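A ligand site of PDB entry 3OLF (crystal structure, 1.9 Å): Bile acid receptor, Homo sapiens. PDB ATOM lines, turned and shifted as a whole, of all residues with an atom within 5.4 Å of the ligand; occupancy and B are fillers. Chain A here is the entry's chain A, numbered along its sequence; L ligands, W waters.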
ATOM      1  N   GLN A  24      -8.498 -11.266 -23.690  1.00  0.00           N
ATOM      2  CA  GLN A  24      -9.396 -11.526 -22.587  1.00  0.00           C
ATOM      3  C   GLN A  24      -8.936 -10.956 -21.292  1.00  0.00           C
ATOM      4  O   GLN A  24      -7.735 -10.781 -21.062  1.00  0.00           O
ATOM      5  CB  GLN A  24      -9.641 -13.017 -22.432  1.00  0.00           C
ATOM      6  CG  GLN A  24     -10.894 -13.441 -23.146  1.00  0.00           C
ATOM      7  CD  GLN A  24     -11.024 -14.933 -23.178  1.00  0.00           C
ATOM      8  OE1 GLN A  24     -12.120 -15.484 -23.062  1.00  0.00           O
ATOM      9  NE2 GLN A  24      -9.900 -15.606 -23.362  1.00  0.00           N
ATOM     10  N   ARG A  25      -9.925 -10.727 -20.394  1.00  0.00           N
ATOM     11  CA  ARG A  25      -9.715 -10.267 -19.031  1.00  0.00           C
ATOM     12  C   ARG A  25      -8.708 -11.244 -18.444  1.00  0.00           C
ATOM     13  O   ARG A  25      -8.926 -12.471 -18.523  1.00  0.00           O
ATOM     14  CB  ARG A  25     -11.038 -10.323 -18.245  1.00  0.00           C
ATOM     15  CG  ARG A  25     -11.180  -9.221 -17.206  1.00  0.00           C
ATOM     16  CD  ARG A  25     -12.627  -9.010 -16.786  1.00  0.00           C
ATOM     17  NE  ARG A  25     -13.143  -7.703 -17.203  1.00  0.00           N
ATOM     18  CZ  ARG A  25     -14.343  -7.224 -16.895  1.00  0.00           C
ATOM     19  NH1 ARG A  25     -15.182  -7.947 -16.153  1.00  0.00           N
ATOM     20  NH2 ARG A  25     -14.724  -6.028 -17.313  1.00  0.00           N
ATOM     21  N   ILE A  30      -9.706 -11.900 -11.806  1.00  0.00           N
ATOM     22  CA  ILE A  30     -10.925 -12.578 -11.368  1.00  0.00           C
ATOM     23  C   ILE A  30     -10.695 -13.357 -10.073  1.00  0.00           C
ATOM     24  O   ILE A  30     -11.483 -13.202  -9.134  1.00  0.00           O
ATOM     25  CB  ILE A  30     -11.490 -13.451 -12.521  1.00  0.00           C
ATOM     26  CG1 ILE A  30     -11.447 -12.668 -13.863  1.00  0.00           C
ATOM     27  CG2 ILE A  30     -12.907 -13.938 -12.174  1.00  0.00           C
ATOM     28  CD1 ILE A  30     -11.194 -13.469 -15.130  1.00  0.00           C
ATOM     29  N   THR A  31      -9.614 -14.161  -9.998  1.00  0.00           N
ATOM     30  CA  THR A  31      -9.299 -14.979  -8.829  1.00  0.00           C
ATOM     31  C   THR A  31      -8.767 -14.188  -7.654  1.00  0.00           C
ATOM     32  O   THR A  31      -9.072 -14.544  -6.527  1.00  0.00           O
ATOM     33  CB  THR A  31      -8.451 -16.184  -9.194  1.00  0.00           C
ATOM     34  OG1 THR A  31      -7.122 -15.758  -9.492  1.00  0.00           O
ATOM     35  CG2 THR A  31      -9.018 -16.949 -10.341  1.00  0.00           C
ATOM     36  N   ILE A  34     -11.909 -12.835  -5.974  1.00  0.00           N
ATOM     37  CA  ILE A  34     -12.697 -13.860  -5.288  1.00  0.00           C
ATOM     38  C   ILE A  34     -11.985 -14.251  -3.993  1.00  0.00           C
ATOM     39  O   ILE A  34     -12.629 -14.422  -2.955  1.00  0.00           O
ATOM     40  CB  ILE A  34     -12.961 -15.093  -6.185  1.00  0.00           C
ATOM     41  CG1 ILE A  34     -13.870 -14.763  -7.380  1.00  0.00           C
ATOM     42  CG2 ILE A  34     -13.553 -16.244  -5.357  1.00  0.00           C
ATOM     43  CD1 ILE A  34     -13.877 -15.814  -8.538  1.00  0.00           C
ATOM     44  N   ASN A  44     -22.190 -11.416  -5.211  1.00  0.00           N
ATOM     45  CA  ASN A  44     -21.674 -12.427  -6.150  1.00  0.00           C
ATOM     46  C   ASN A  44     -22.511 -12.554  -7.407  1.00  0.00           C
ATOM     47  O   ASN A  44     -21.963 -12.767  -8.493  1.00  0.00           O
ATOM     48  CB  ASN A  44     -21.516 -13.776  -5.478  1.00  0.00           C
ATOM     49  CG  ASN A  44     -20.320 -13.872  -4.552  1.00  0.00           C
ATOM     50  OD1 ASN A  44     -20.403 -14.418  -3.457  1.00  0.00           O
ATOM     51  ND2 ASN A  44     -19.180 -13.345  -4.961  1.00  0.00           N
ATOM     52  N   ILE A  47     -21.414  -9.718  -9.427  1.00  0.00           N
ATOM     53  CA  ILE A  47     -20.072  -9.945  -9.985  1.00  0.00           C
ATOM     54  C   ILE A  47     -20.283 -10.867 -11.212  1.00  0.00           C
ATOM     55  O   ILE A  47     -19.744 -10.589 -12.280  1.00  0.00           O
ATOM     56  CB  ILE A  47     -19.082 -10.549  -8.951  1.00  0.00           C
ATOM     57  CG1 ILE A  47     -18.680  -9.507  -7.893  1.00  0.00           C
ATOM     58  CG2 ILE A  47     -17.804 -11.095  -9.665  1.00  0.00           C
ATOM     59  CD1 ILE A  47     -18.197 -10.115  -6.574  1.00  0.00           C
ATOM     60  N   LEU A  48     -21.105 -11.891 -11.059  1.00  0.00           N
ATOM     61  CA  LEU A  48     -21.390 -12.824 -12.161  1.00  0.00           C
ATOM     62  C   LEU A  48     -22.017 -12.135 -13.382  1.00  0.00           C
ATOM     63  O   LEU A  48     -21.575 -12.386 -14.501  1.00  0.00           O
ATOM     64  CB  LEU A  48     -22.253 -14.026 -11.677  1.00  0.00           C
ATOM     65  CG  LEU A  48     -22.884 -14.957 -12.769  1.00  0.00           C
ATOM     66  CD1 LEU A  48     -21.824 -15.753 -13.570  1.00  0.00           C
ATOM     67  CD2 LEU A  48     -23.893 -15.918 -12.131  1.00  0.00           C
ATOM     68  N   MET A  51     -19.260  -9.881 -15.076  1.00  0.00           N
ATOM     69  CA  MET A  51     -18.261 -10.736 -15.702  1.00  0.00           C
ATOM     70  C   MET A  51     -18.813 -11.396 -16.952  1.00  0.00           C
ATOM     71  O   MET A  51     -18.100 -11.500 -17.950  1.00  0.00           O
ATOM     72  CB  MET A  51     -17.792 -11.850 -14.744  1.00  0.00           C
ATOM     73  CG  MET A  51     -16.878 -11.378 -13.600  1.00  0.00           C
ATOM     74  SD  MET A  51     -15.312 -10.781 -14.215  1.00  0.00           S
ATOM     75  CE  MET A  51     -14.588 -12.264 -14.749  1.00  0.00           C
ATOM     76  N   ALA A  52     -20.068 -11.891 -16.896  1.00  0.00           N
ATOM     77  CA  ALA A  52     -20.694 -12.608 -17.997  1.00  0.00           C
ATOM     78  C   ALA A  52     -21.060 -11.686 -19.150  1.00  0.00           C
ATOM     79  O   ALA A  52     -20.952 -12.104 -20.295  1.00  0.00           O
ATOM     80  CB  ALA A  52     -21.912 -13.384 -17.536  1.00  0.00           C
ATOM     81  N   ASN A  54     -19.334  -8.841 -19.885  1.00  0.00           N
ATOM     82  CA  ASN A  54     -18.061  -8.515 -20.542  1.00  0.00           C
ATOM     83  C   ASN A  54     -17.585  -9.706 -21.401  1.00  0.00           C
ATOM     84  O   ASN A  54     -17.113  -9.514 -22.524  1.00  0.00           O
ATOM     85  CB  ASN A  54     -16.982  -8.125 -19.520  1.00  0.00           C
ATOM     86  CG  ASN A  54     -15.641  -7.932 -20.169  1.00  0.00           C
ATOM     87  OD1 ASN A  54     -14.742  -8.794 -20.095  1.00  0.00           O
ATOM     88  ND2 ASN A  54     -15.498  -6.866 -20.933  1.00  0.00           N
ATOM     89  N   HIS A  55     -17.744 -10.940 -20.863  1.00  0.00           N
ATOM     90  CA  HIS A  55     -17.379 -12.159 -21.575  1.00  0.00           C
ATOM     91  C   HIS A  55     -18.154 -12.303 -22.888  1.00  0.00           C
ATOM     92  O   HIS A  55     -17.542 -12.659 -23.896  1.00  0.00           O
ATOM     93  CB  HIS A  55     -17.600 -13.410 -20.692  1.00  0.00           C
ATOM     94  CG  HIS A  55     -17.254 -14.683 -21.402  1.00  0.00           C
ATOM     95  ND1 HIS A  55     -18.221 -15.426 -22.033  1.00  0.00           N
ATOM     96  CD2 HIS A  55     -16.047 -15.265 -21.594  1.00  0.00           C
ATOM     97  CE1 HIS A  55     -17.577 -16.432 -22.609  1.00  0.00           C
ATOM     98  NE2 HIS A  55     -16.276 -16.397 -22.375  1.00  0.00           N
ATOM     99  N   MET A  89     -18.395 -19.649 -21.805  1.00  0.00           N
ATOM    100  CA  MET A  89     -18.297 -19.097 -20.487  1.00  0.00           C
ATOM    101  C   MET A  89     -17.856 -20.157 -19.435  1.00  0.00           C
ATOM    102  O   MET A  89     -16.884 -19.906 -18.722  1.00  0.00           O
ATOM    103  CB  MET A  89     -19.568 -18.364 -20.115  1.00  0.00           C
ATOM    104  CG  MET A  89     -19.403 -17.568 -18.885  1.00  0.00           C
ATOM    105  SD  MET A  89     -19.950 -18.515 -17.464  1.00  0.00           S
ATOM    106  CE  MET A  89     -21.572 -17.870 -17.341  1.00  0.00           C
ATOM    107  N   PHE A  90     -18.498 -21.339 -19.407  1.00  0.00           N
ATOM    108  CA  PHE A  90     -18.091 -22.407 -18.503  1.00  0.00           C
ATOM    109  C   PHE A  90     -16.714 -22.956 -18.839  1.00  0.00           C
ATOM    110  O   PHE A  90     -15.980 -23.290 -17.925  1.00  0.00           O
ATOM    111  CB  PHE A  90     -19.138 -23.553 -18.435  1.00  0.00           C
ATOM    112  CG  PHE A  90     -20.296 -23.203 -17.546  1.00  0.00           C
ATOM    113  CD1 PHE A  90     -20.122 -23.052 -16.168  1.00  0.00           C
ATOM    114  CD2 PHE A  90     -21.549 -22.946 -18.083  1.00  0.00           C
ATOM    115  CE1 PHE A  90     -21.187 -22.679 -15.362  1.00  0.00           C
ATOM    116  CE2 PHE A  90     -22.624 -22.569 -17.268  1.00  0.00           C
ATOM    117  CZ  PHE A  90     -22.434 -22.456 -15.911  1.00  0.00           C
ATOM    118  N   ARG A  92     -14.178 -21.232 -20.183  1.00  0.00           N
ATOM    119  CA  ARG A  92     -13.324 -20.173 -19.692  1.00  0.00           C
ATOM    120  C   ARG A  92     -13.259 -20.200 -18.128  1.00  0.00           C
ATOM    121  O   ARG A  92     -12.180 -20.103 -17.564  1.00  0.00           O
ATOM    122  CB  ARG A  92     -13.854 -18.819 -20.209  1.00  0.00           C
ATOM    123  CG  ARG A  92     -13.083 -17.604 -19.706  1.00  0.00           C
ATOM    124  CD  ARG A  92     -11.591 -17.667 -20.019  1.00  0.00           C
ATOM    125  NE  ARG A  92     -10.926 -16.444 -19.572  1.00  0.00           N
ATOM    126  CZ  ARG A  92      -9.658 -16.150 -19.789  1.00  0.00           C
ATOM    127  NH1 ARG A  92      -8.878 -16.992 -20.462  1.00  0.00           N
ATOM    128  NH2 ARG A  92      -9.151 -15.007 -19.363  1.00  0.00           N
ATOM    129  N   SER A  93     -14.398 -20.429 -17.455  1.00  0.00           N
ATOM    130  CA  SER A  93     -14.390 -20.542 -15.984  1.00  0.00           C
ATOM    131  C   SER A  93     -13.573 -21.778 -15.587  1.00  0.00           C
ATOM    132  O   SER A  93     -12.777 -21.717 -14.650  1.00  0.00           O
ATOM    133  CB  SER A  93     -15.805 -20.649 -15.433  1.00  0.00           C
ATOM    134  OG  SER A  93     -16.553 -19.465 -15.670  1.00  0.00           O
ATOM    135  N   ALA A  94     -13.684 -22.886 -16.373  1.00  0.00           N
ATOM    136  CA  ALA A  94     -12.907 -24.110 -16.128  1.00  0.00           C
ATOM    137  C   ALA A  94     -11.417 -23.822 -16.241  1.00  0.00           C
ATOM    138  O   ALA A  94     -10.649 -24.235 -15.389  1.00  0.00           O
ATOM    139  CB  ALA A  94     -13.311 -25.223 -17.094  1.00  0.00           C
ATOM    140  N   ILE A  96      -9.733 -20.925 -15.823  1.00  0.00           N
ATOM    141  CA  ILE A  96      -9.305 -20.130 -14.677  1.00  0.00           C
ATOM    142  C   ILE A  96      -9.246 -20.972 -13.392  1.00  0.00           C
ATOM    143  O   ILE A  96      -8.278 -20.844 -12.638  1.00  0.00           O
ATOM    144  CB  ILE A  96     -10.194 -18.879 -14.553  1.00  0.00           C
ATOM    145  CG1 ILE A  96      -9.906 -17.910 -15.718  1.00  0.00           C
ATOM    146  CG2 ILE A  96      -9.972 -18.182 -13.204  1.00  0.00           C
ATOM    147  CD1 ILE A  96     -10.982 -16.981 -16.013  1.00  0.00           C
ATOM    148  N   PHE A  97     -10.255 -21.825 -13.176  1.00  0.00           N
ATOM    149  CA  PHE A  97     -10.330 -22.681 -11.984  1.00  0.00           C
ATOM    150  C   PHE A  97      -9.093 -23.580 -11.832  1.00  0.00           C
ATOM    151  O   PHE A  97      -8.633 -23.779 -10.711  1.00  0.00           O
ATOM    152  CB  PHE A  97     -11.596 -23.525 -11.992  1.00  0.00           C
ATOM    153  CG  PHE A  97     -11.832 -24.329 -10.732  1.00  0.00           C
ATOM    154  CD1 PHE A  97     -12.513 -23.772  -9.644  1.00  0.00           C
ATOM    155  CD2 PHE A  97     -11.447 -25.668 -10.645  1.00  0.00           C
ATOM    156  CE1 PHE A  97     -12.753 -24.532  -8.492  1.00  0.00           C
ATOM    157  CE2 PHE A  97     -11.689 -26.420  -9.500  1.00  0.00           C
ATOM    158  CZ  PHE A  97     -12.333 -25.847  -8.420  1.00  0.00           C
ATOM    159  N   LEU A 109     -10.409 -20.888  -3.330  1.00  0.00           N
ATOM    160  CA  LEU A 109     -11.164 -20.458  -4.495  1.00  0.00           C
ATOM    161  C   LEU A 109     -12.399 -21.334  -4.652  1.00  0.00           C
ATOM    162  O   LEU A 109     -13.508 -20.809  -4.809  1.00  0.00           O
ATOM    163  CB  LEU A 109     -10.292 -20.450  -5.762  1.00  0.00           C
ATOM    164  CG  LEU A 109     -11.017 -20.096  -7.068  1.00  0.00           C
ATOM    165  CD1 LEU A 109     -11.378 -18.619  -7.117  1.00  0.00           C
ATOM    166  CD2 LEU A 109     -10.215 -20.525  -8.277  1.00  0.00           C
ATOM    167  N   ILE A 113     -16.505 -20.149  -4.274  1.00  0.00           N
ATOM    168  CA  ILE A 113     -17.443 -20.399  -5.374  1.00  0.00           C
ATOM    169  C   ILE A 113     -18.612 -21.260  -4.905  1.00  0.00           C
ATOM    170  O   ILE A 113     -19.771 -20.965  -5.209  1.00  0.00           O
ATOM    171  CB  ILE A 113     -16.705 -21.008  -6.580  1.00  0.00           C
ATOM    172  CG1 ILE A 113     -15.681 -20.008  -7.157  1.00  0.00           C
ATOM    173  CG2 ILE A 113     -17.699 -21.475  -7.660  1.00  0.00           C
ATOM    174  CD1 ILE A 113     -14.791 -20.576  -8.175  1.00  0.00           C
ATOM    175  N   SER A 116     -20.977 -19.136  -3.077  1.00  0.00           N
ATOM    176  CA  SER A 116     -21.290 -17.885  -3.793  1.00  0.00           C
ATOM    177  C   SER A 116     -22.777 -17.541  -3.882  1.00  0.00           C
ATOM    178  O   SER A 116     -23.112 -16.374  -4.122  1.00  0.00           O
ATOM    179  CB  SER A 116     -20.685 -17.899  -5.188  1.00  0.00           C
ATOM    180  OG  SER A 116     -21.340 -18.857  -6.010  1.00  0.00           O
ATOM    181  N   ILE A 118     -25.001 -19.958  -5.666  1.00  0.00           N
ATOM    182  CA  ILE A 118     -25.558 -21.001  -6.527  1.00  0.00           C
ATOM    183  C   ILE A 118     -26.165 -22.119  -5.636  1.00  0.00           C
ATOM    184  O   ILE A 118     -25.640 -22.395  -4.551  1.00  0.00           O
ATOM    185  CB  ILE A 118     -24.492 -21.522  -7.523  1.00  0.00           C
ATOM    186  CG1 ILE A 118     -25.075 -22.566  -8.511  1.00  0.00           C
ATOM    187  CG2 ILE A 118     -23.235 -22.005  -6.814  1.00  0.00           C
ATOM    188  CD1 ILE A 118     -24.500 -23.875  -8.363  1.00  0.00           C
ATOM    189  N   MET A 126     -21.105 -28.763 -11.711  1.00  0.00           N
ATOM    190  CA  MET A 126     -20.118 -27.740 -12.083  1.00  0.00           C
ATOM    191  C   MET A 126     -18.666 -28.102 -11.709  1.00  0.00           C
ATOM    192  O   MET A 126     -17.777 -28.038 -12.563  1.00  0.00           O
ATOM    193  CB  MET A 126     -20.551 -26.382 -11.535  1.00  0.00           C
ATOM    194  CG  MET A 126     -19.505 -25.307 -11.726  1.00  0.00           C
ATOM    195  SD  MET A 126     -19.990 -23.715 -11.046  1.00  0.00           S
ATOM    196  CE  MET A 126     -19.995 -24.058  -9.302  1.00  0.00           C
ATOM    197  N   TYR A 130     -15.346 -28.968 -13.978  1.00  0.00           N
ATOM    198  CA  TYR A 130     -14.048 -28.295 -13.836  1.00  0.00           C
ATOM    199  C   TYR A 130     -12.962 -29.261 -13.474  1.00  0.00           C
ATOM    200  O   TYR A 130     -11.812 -29.075 -13.875  1.00  0.00           O
ATOM    201  CB  TYR A 130     -14.067 -27.194 -12.770  1.00  0.00           C
ATOM    202  CG  TYR A 130     -15.021 -26.050 -13.012  1.00  0.00           C
ATOM    203  CD1 TYR A 130     -15.592 -25.834 -14.259  1.00  0.00           C
ATOM    204  CD2 TYR A 130     -15.316 -25.152 -11.988  1.00  0.00           C
ATOM    205  CE1 TYR A 130     -16.468 -24.772 -14.481  1.00  0.00           C
ATOM    206  CE2 TYR A 130     -16.183 -24.082 -12.202  1.00  0.00           C
ATOM    207  CZ  TYR A 130     -16.756 -23.903 -13.446  1.00  0.00           C
ATOM    208  OH  TYR A 130     -17.662 -22.882 -13.628  1.00  0.00           O
ATOM    209  N   MET A 211     -30.312 -22.664 -13.118  1.00  0.00           N
ATOM    210  CA  MET A 211     -29.133 -22.452 -12.289  1.00  0.00           C
ATOM    211  C   MET A 211     -29.008 -20.999 -11.876  1.00  0.00           C
ATOM    212  O   MET A 211     -28.579 -20.710 -10.749  1.00  0.00           O
ATOM    213  CB  MET A 211     -27.908 -22.910 -13.089  1.00  0.00           C
ATOM    214  CG  MET A 211     -26.629 -22.992 -12.304  1.00  0.00           C
ATOM    215  SD  MET A 211     -25.260 -23.559 -13.370  1.00  0.00           S
ATOM    216  CE  MET A 211     -26.064 -24.898 -14.285  1.00  0.00           C
ATOM    217  N   LEU A 212     -29.331 -20.087 -12.791  1.00  0.00           N
ATOM    218  CA  LEU A 212     -29.284 -18.645 -12.566  1.00  0.00           C
ATOM    219  C   LEU A 212     -30.458 -18.182 -11.727  1.00  0.00           C
ATOM    220  O   LEU A 212     -30.275 -17.391 -10.806  1.00  0.00           O
ATOM    221  CB  LEU A 212     -29.319 -17.935 -13.912  1.00  0.00           C
ATOM    222  CG  LEU A 212     -28.076 -18.102 -14.791  1.00  0.00           C
ATOM    223  CD1 LEU A 212     -28.413 -17.771 -16.212  1.00  0.00           C
ATOM    224  CD2 LEU A 212     -26.896 -17.269 -14.243  1.00  0.00           C
ATOM    225  N   TRP A 215     -30.227 -18.932  -8.000  1.00  0.00           N
ATOM    226  CA  TRP A 215     -29.246 -18.255  -7.143  1.00  0.00           C
ATOM    227  C   TRP A 215     -29.958 -17.711  -5.897  1.00  0.00           C
ATOM    228  O   TRP A 215     -31.059 -17.161  -6.009  1.00  0.00           O
ATOM    229  CB  TRP A 215     -28.577 -17.114  -7.892  1.00  0.00           C
ATOM    230  CG  TRP A 215     -27.195 -16.820  -7.417  1.00  0.00           C
ATOM    231  CD1 TRP A 215     -26.827 -16.013  -6.387  1.00  0.00           C
ATOM    232  CD2 TRP A 215     -25.976 -17.260  -8.029  1.00  0.00           C
ATOM    233  NE1 TRP A 215     -25.456 -15.904  -6.327  1.00  0.00           N
ATOM    234  CE2 TRP A 215     -24.909 -16.679  -7.304  1.00  0.00           C
ATOM    235  CE3 TRP A 215     -25.678 -18.090  -9.131  1.00  0.00           C
ATOM    236  CZ2 TRP A 215     -23.565 -16.916  -7.627  1.00  0.00           C
ATOM    237  CZ3 TRP A 215     -24.351 -18.340  -9.433  1.00  0.00           C
ATOM    238  CH2 TRP A 215     -23.307 -17.749  -8.705  1.00  0.00           C
HETATM  239  N1  LIG L   1     -17.253 -18.422 -12.057  1.00  0.00           N
HETATM  240  C1  LIG L   1     -17.903 -19.613 -12.237  1.00  0.00           C
HETATM  241  N2  LIG L   1     -17.077 -20.606 -12.110  1.00  0.00           N
HETATM  242  C2  LIG L   1     -15.937 -18.703 -11.834  1.00  0.00           C
HETATM  243  C3  LIG L   1     -15.850 -20.114 -11.879  1.00  0.00           C
HETATM  244  C4  LIG L   1     -17.181 -16.205 -13.146  1.00  0.00           C
HETATM  245  C5  LIG L   1     -17.882 -17.095 -12.149  1.00  0.00           C
HETATM  246  C6  LIG L   1     -14.825 -17.912 -11.615  1.00  0.00           C
HETATM  247  N3  LIG L   1     -16.751 -16.798 -14.285  1.00  0.00           N
HETATM  248  C7  LIG L   1     -14.600 -20.719 -11.670  1.00  0.00           C
HETATM  249  C8  LIG L   1     -13.614 -18.525 -11.405  1.00  0.00           C
HETATM  250  C9  LIG L   1     -16.075 -16.140 -15.323  1.00  0.00           C
HETATM  251  C10 LIG L   1     -13.965 -14.192 -18.495  1.00  0.00           C
HETATM  252  C11 LIG L   1     -19.339 -19.703 -12.532  1.00  0.00           C
HETATM  253  C12 LIG L   1     -13.511 -19.912 -11.440  1.00  0.00           C
HETATM  254  C13 LIG L   1     -14.696 -14.863 -17.391  1.00  0.00           C
HETATM  255  C14 LIG L   1     -16.089 -14.730 -17.283  1.00  0.00           C
HETATM  256  C15 LIG L   1     -16.786 -15.389 -16.273  1.00  0.00           C
HETATM  257  O1  LIG L   1     -16.989 -15.023 -12.935  1.00  0.00           O
HETATM  258  O2  LIG L   1     -12.795 -14.406 -18.718  1.00  0.00           O
HETATM  259  C16 LIG L   1     -14.682 -16.273 -15.430  1.00  0.00           C
HETATM  260  C17 LIG L   1     -14.001 -15.639 -16.449  1.00  0.00           C
HETATM  261  C18 LIG L   1     -18.387 -16.538 -10.802  1.00  0.00           C
HETATM  262  C19 LIG L   1     -20.210 -20.167 -11.550  1.00  0.00           C
HETATM  263  C20 LIG L   1     -19.824 -19.260 -13.765  1.00  0.00           C
HETATM  264  F1  LIG L   1     -12.505 -17.806 -11.144  1.00  0.00           F
HETATM  265  F2  LIG L   1     -12.308 -20.438 -11.247  1.00  0.00           F
HETATM  266  O3  LIG L   1     -14.612 -13.318 -19.291  1.00  0.00           O
HETATM  267  C21 LIG L   1     -22.049 -19.809 -13.048  1.00  0.00           C
HETATM  268  C22 LIG L   1     -21.569 -20.230 -11.819  1.00  0.00           C
HETATM  269  C23 LIG L   1     -21.187 -19.297 -14.016  1.00  0.00           C
HETATM  270 CL1  LIG L   1     -23.767 -19.874 -13.356  1.00  0.00          CL
HETATM  271  C24 LIG L   1     -18.297 -15.228 -16.175  1.00  0.00           C
HETATM  272  C25 LIG L   1     -18.099 -17.418  -9.588  1.00  0.00           C
HETATM  273  C26 LIG L   1     -18.119 -15.066 -10.525  1.00  0.00           C
HETATM  274  C27 LIG L   1     -18.953 -14.585  -9.322  1.00  0.00           C
HETATM  275  C28 LIG L   1     -18.967 -16.971  -8.401  1.00  0.00           C
HETATM  276  C29 LIG L   1     -18.751 -15.485  -8.090  1.00  0.00           C
HETATM  277  O   HOH W   1     -15.461 -11.025 -18.213  1.00  0.00           O
HETATM  278  O   HOH W   2     -13.134 -13.164 -21.419  1.00  0.00           O
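N2 of the ligand is in hydrogen-bond range of OH of Tyr 130.
NE of Arg 92 is in salt-bridge range of O2 of the ligand, 2.9 Å away.
OG of Ser 93 lies within hydrogen-bond range of N3 of the ligand (3.0 Å).
The side-chain hydroxyl (OH) of Tyr 130 is in hydrogen-bond range of the side-chain sulfur (SD) of Met 126, 3.6 Å away.
The guanidinium group of Arg 92 lies within hydrogen-bond range of the backbone carbonyl oxygen of Arg 25 (2.7 Å).
The guanidinium group (NH1) of Arg 92 lies close to the side-chain amide nitrogen (NE2) of Gln 24 (3.4 Å).
The side-chain hydroxyl (OG) of Ser 93 lies within hydrogen-bond range of the backbone carbonyl oxygen (O) of Met 89.
O of Ile 113 sits at hydrogen-bond distance from OG of Ser 116 (2.7 Å).
The backbone carbonyl oxygen (O) of Ser 116 sits close to the side-chain amide oxygen (OD1) of Asn 44, at 3.4 Å.
The guanidinium group (NH1) of Arg 25 lies within hydrogen-bond range of the side-chain sulfur (SD) of Met 51.
The backbone carbonyl oxygen (O) of Ser 116 lies within hydrogen-bond range of the indole nitrogen (NE1) of Trp 215.
The backbone NH (N) of Phe 97 sits close to a fluorine (F2) of the ligand, at 3.1 Å.
CD1 of Ile 30 touches C17 of the ligand, at 3.8 Å.
CG2 of Thr 31 touches F1 of the ligand (3.7 Å).
CD1 of Ile 34 touches F1 of the ligand, at 3.6 Å.
O of Asn 44 touches C27 of the ligand (3.6 Å).
Ile 47 touches the ligand.
CD1 of Leu 48 touches C23 of the ligand, at 3.6 Å.
Met 51 touches the ligand.
Ala 52 touches the ligand.
His 55 touches the ligand.
CE of Met 89 touches C23 of the ligand (3.6 Å).
CE1 of Phe 90 touches C23 of the ligand, 3.6 Å away.
CG2 of Ile 96 touches F1 of the ligand, 3.3 Å away.
Leu 109 touches the ligand.
Ile 113 touches the ligand.
CB of Ser 116 touches C28 of the ligand, 3.8 Å away.
Met 126 touches the ligand (SD to C19, 3.6 Å).
SD of Met 211 touches CL1 of the ligand, 3.98 Å away.
Hydrophobic or aromatic side chains within 4 Å of the ligand: Ile 30, Ile 34, Ile 47, Leu 48, Met 51, His 55, Met 89, Phe 90, Ile 96, Phe 97, Leu 109, Ile 113, Met 126, Tyr 130 and Met 211.
The nearest printed residue that does not touch the ligand is Trp 215 (4.1 Å).
Water W2 lies within hydrogen-bond range of O3 of the ligand (2.6 Å) and OE1 of Gln 24 (3.0 Å).
Water W1 lies within hydrogen-bond range of O3 of the ligand, O of Met 51, OD1 of Asn 54 and N of His 55.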
